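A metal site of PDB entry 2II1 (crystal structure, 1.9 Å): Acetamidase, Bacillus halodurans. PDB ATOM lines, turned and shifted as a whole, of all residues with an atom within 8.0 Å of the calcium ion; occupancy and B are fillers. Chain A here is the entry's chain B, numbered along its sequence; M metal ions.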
ATOM      1  N   ALA A 247      26.603 -10.581 -15.221  1.00  0.00           N
ATOM      2  CA  ALA A 247      26.155  -9.479 -16.115  1.00  0.00           C
ATOM      3  C   ALA A 247      26.268  -8.111 -15.438  1.00  0.00           C
ATOM      4  O   ALA A 247      26.795  -7.151 -15.986  1.00  0.00           O
ATOM      5  CB  ALA A 247      24.682  -9.703 -16.553  1.00  0.00           C
ATOM      6  N   THR A 248      25.748  -8.009 -14.234  1.00  0.00           N
ATOM      7  CA  THR A 248      25.743  -6.753 -13.546  1.00  0.00           C
ATOM      8  C   THR A 248      27.171  -6.324 -13.164  1.00  0.00           C
ATOM      9  O   THR A 248      27.478  -5.148 -13.283  1.00  0.00           O
ATOM     10  CB  THR A 248      24.843  -6.800 -12.305  1.00  0.00           C
ATOM     11  OG1 THR A 248      25.260  -7.881 -11.463  1.00  0.00           O
ATOM     12  CG2 THR A 248      23.406  -6.985 -12.700  1.00  0.00           C
ATOM     13  N   PHE A 249      28.009  -7.268 -12.727  1.00  0.00           N
ATOM     14  CA  PHE A 249      29.454  -7.036 -12.520  1.00  0.00           C
ATOM     15  C   PHE A 249      30.205  -6.538 -13.792  1.00  0.00           C
ATOM     16  O   PHE A 249      30.947  -5.550 -13.756  1.00  0.00           O
ATOM     17  CB  PHE A 249      30.118  -8.317 -11.976  1.00  0.00           C
ATOM     18  CG  PHE A 249      31.628  -8.282 -11.967  1.00  0.00           C
ATOM     19  CD1 PHE A 249      32.310  -7.225 -11.368  1.00  0.00           C
ATOM     20  CD2 PHE A 249      32.367  -9.303 -12.539  1.00  0.00           C
ATOM     21  CE1 PHE A 249      33.712  -7.174 -11.361  1.00  0.00           C
ATOM     22  CE2 PHE A 249      33.770  -9.265 -12.526  1.00  0.00           C
ATOM     23  CZ  PHE A 249      34.443  -8.193 -11.945  1.00  0.00           C
ATOM     24  N   LEU A 250      30.004  -7.243 -14.896  1.00  0.00           N
ATOM     25  CA  LEU A 250      30.629  -6.909 -16.169  1.00  0.00           C
ATOM     26  C   LEU A 250      30.070  -5.576 -16.750  1.00  0.00           C
ATOM     27  O   LEU A 250      30.807  -4.798 -17.333  1.00  0.00           O
ATOM     28  CB  LEU A 250      30.461  -8.136 -17.105  1.00  0.00           C
ATOM     29  CG  LEU A 250      31.076  -8.333 -18.494  1.00  0.00           C
ATOM     30  CD1 LEU A 250      32.612  -8.322 -18.490  1.00  0.00           C
ATOM     31  CD2 LEU A 250      30.546  -9.662 -19.044  1.00  0.00           C
ATOM     32  N   ALA A 251      28.789  -5.275 -16.540  1.00  0.00           N
ATOM     33  CA  ALA A 251      28.259  -3.972 -16.920  1.00  0.00           C
ATOM     34  C   ALA A 251      28.854  -2.913 -16.019  1.00  0.00           C
ATOM     35  O   ALA A 251      29.404  -1.911 -16.481  1.00  0.00           O
ATOM     36  CB  ALA A 251      26.738  -3.953 -16.844  1.00  0.00           C
ATOM     37  N   ASN A 252      28.731  -3.125 -14.706  1.00  0.00           N
ATOM     38  CA  ASN A 252      29.196  -2.152 -13.721  1.00  0.00           C
ATOM     39  C   ASN A 252      30.675  -1.774 -13.842  1.00  0.00           C
ATOM     40  O   ASN A 252      31.013  -0.615 -13.700  1.00  0.00           O
ATOM     41  CB  ASN A 252      28.911  -2.628 -12.281  1.00  0.00           C
ATOM     42  CG  ASN A 252      27.420  -2.591 -11.919  1.00  0.00           C
ATOM     43  OD1 ASN A 252      26.648  -1.813 -12.455  1.00  0.00           O
ATOM     44  ND2 ASN A 252      27.017  -3.447 -10.980  1.00  0.00           N
ATOM     45  N   ARG A 253      31.539  -2.747 -14.111  1.00  0.00           N
ATOM     46  CA  ARG A 253      32.999  -2.538 -14.074  1.00  0.00           C
ATOM     47  C   ARG A 253      33.662  -2.296 -15.431  1.00  0.00           C
ATOM     48  O   ARG A 253      34.872  -2.023 -15.489  1.00  0.00           O
ATOM     49  CB  ARG A 253      33.684  -3.708 -13.362  1.00  0.00           C
ATOM     50  CG  ARG A 253      33.517  -3.690 -11.834  1.00  0.00           C
ATOM     51  N   THR A 254      32.883  -2.334 -16.513  1.00  0.00           N
ATOM     52  CA  THR A 254      33.375  -2.233 -17.881  1.00  0.00           C
ATOM     53  C   THR A 254      32.617  -1.172 -18.682  1.00  0.00           C
ATOM     54  O   THR A 254      31.501  -0.743 -18.305  1.00  0.00           O
ATOM     55  CB  THR A 254      33.197  -3.602 -18.635  1.00  0.00           C
ATOM     56  OG1 THR A 254      33.628  -4.700 -17.798  1.00  0.00           O
ATOM     57  CG2 THR A 254      33.984  -3.628 -19.914  1.00  0.00           C
ATOM     58  N   ALA A 255      33.193  -0.811 -19.822  1.00  0.00           N
ATOM     59  CA  ALA A 255      32.575   0.064 -20.793  1.00  0.00           C
ATOM     60  C   ALA A 255      31.329  -0.555 -21.426  1.00  0.00           C
ATOM     61  O   ALA A 255      30.596   0.117 -22.128  1.00  0.00           O
ATOM     62  CB  ALA A 255      33.569   0.409 -21.876  1.00  0.00           C
ATOM     63  N   LEU A 256      31.091  -1.836 -21.173  1.00  0.00           N
ATOM     64  CA  LEU A 256      29.925  -2.483 -21.727  1.00  0.00           C
ATOM     65  C   LEU A 256      28.674  -1.985 -21.029  1.00  0.00           C
ATOM     66  O   LEU A 256      28.688  -1.786 -19.811  1.00  0.00           O
ATOM     67  CB  LEU A 256      30.011  -4.005 -21.502  1.00  0.00           C
ATOM     68  CG  LEU A 256      31.155  -4.782 -22.113  1.00  0.00           C
ATOM     69  CD1 LEU A 256      30.868  -6.278 -21.878  1.00  0.00           C
ATOM     70  CD2 LEU A 256      31.356  -4.505 -23.615  1.00  0.00           C
ATOM     71  N   SER A 257      27.593  -1.847 -21.788  1.00  0.00           N
ATOM     72  CA  SER A 257      26.246  -1.706 -21.239  1.00  0.00           C
ATOM     73  C   SER A 257      25.749  -3.046 -20.740  1.00  0.00           C
ATOM     74  O   SER A 257      26.362  -4.089 -21.005  1.00  0.00           O
ATOM     75  CB  SER A 257      25.308  -1.218 -22.324  1.00  0.00           C
ATOM     76  OG  SER A 257      25.253  -2.196 -23.348  1.00  0.00           O
ATOM     77  N   ILE A 258      24.627  -3.029 -20.037  1.00  0.00           N
ATOM     78  CA  ILE A 258      24.005  -4.261 -19.538  1.00  0.00           C
ATOM     79  C   ILE A 258      23.552  -5.112 -20.702  1.00  0.00           C
ATOM     80  O   ILE A 258      23.582  -6.330 -20.638  1.00  0.00           O
ATOM     81  CB  ILE A 258      22.825  -3.963 -18.558  1.00  0.00           C
ATOM     82  CG1 ILE A 258      22.391  -5.240 -17.815  1.00  0.00           C
ATOM     83  CG2 ILE A 258      21.674  -3.266 -19.280  1.00  0.00           C
ATOM     84  CD1 ILE A 258      23.511  -5.894 -16.961  1.00  0.00           C
ATOM     85  N   GLU A 260      25.171  -5.088 -23.746  1.00  0.00           N
ATOM     86  CA  GLU A 260      26.400  -5.634 -24.324  1.00  0.00           C
ATOM     87  C   GLU A 260      26.992  -6.744 -23.452  1.00  0.00           C
ATOM     88  O   GLU A 260      27.501  -7.741 -23.957  1.00  0.00           O
ATOM     89  CB  GLU A 260      27.418  -4.523 -24.518  1.00  0.00           C
ATOM     90  CG  GLU A 260      27.034  -3.551 -25.616  1.00  0.00           C
ATOM     91  CD  GLU A 260      27.982  -2.400 -25.729  1.00  0.00           C
ATOM     92  OE1 GLU A 260      28.391  -1.877 -24.693  1.00  0.00           O
ATOM     93  OE2 GLU A 260      28.302  -2.023 -26.864  1.00  0.00           O
ATOM     94  N   ALA A 261      26.893  -6.577 -22.136  1.00  0.00           N
ATOM     95  CA  ALA A 261      27.259  -7.644 -21.188  1.00  0.00           C
ATOM     96  C   ALA A 261      26.433  -8.937 -21.416  1.00  0.00           C
ATOM     97  O   ALA A 261      26.986 -10.033 -21.484  1.00  0.00           O
ATOM     98  CB  ALA A 261      27.126  -7.129 -19.739  1.00  0.00           C
HETATM   99 CA    CA M   1      29.119  -0.172 -18.160  1.00  0.00          CA
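The side-chain hydroxyl of Thr 254 is in hydrogen-bond range of the backbone carbonyl oxygen of Leu 250.
Residues that only touch the calcium ion: Ala 255. Within 4 Å of the calcium ion: Ala 251, Thr 254, Ala 255 and Leu 256.
The calcium ion is bound by O of Leu 256 (2.3 Å). The calcium ion is bound by the backbone carbonyl oxygen (O) of Ala 251, 2.4 Å away. O of Thr 254 binds the calcium ion, at 2.5 Å. The calcium ion has three donor atoms within binding distance.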
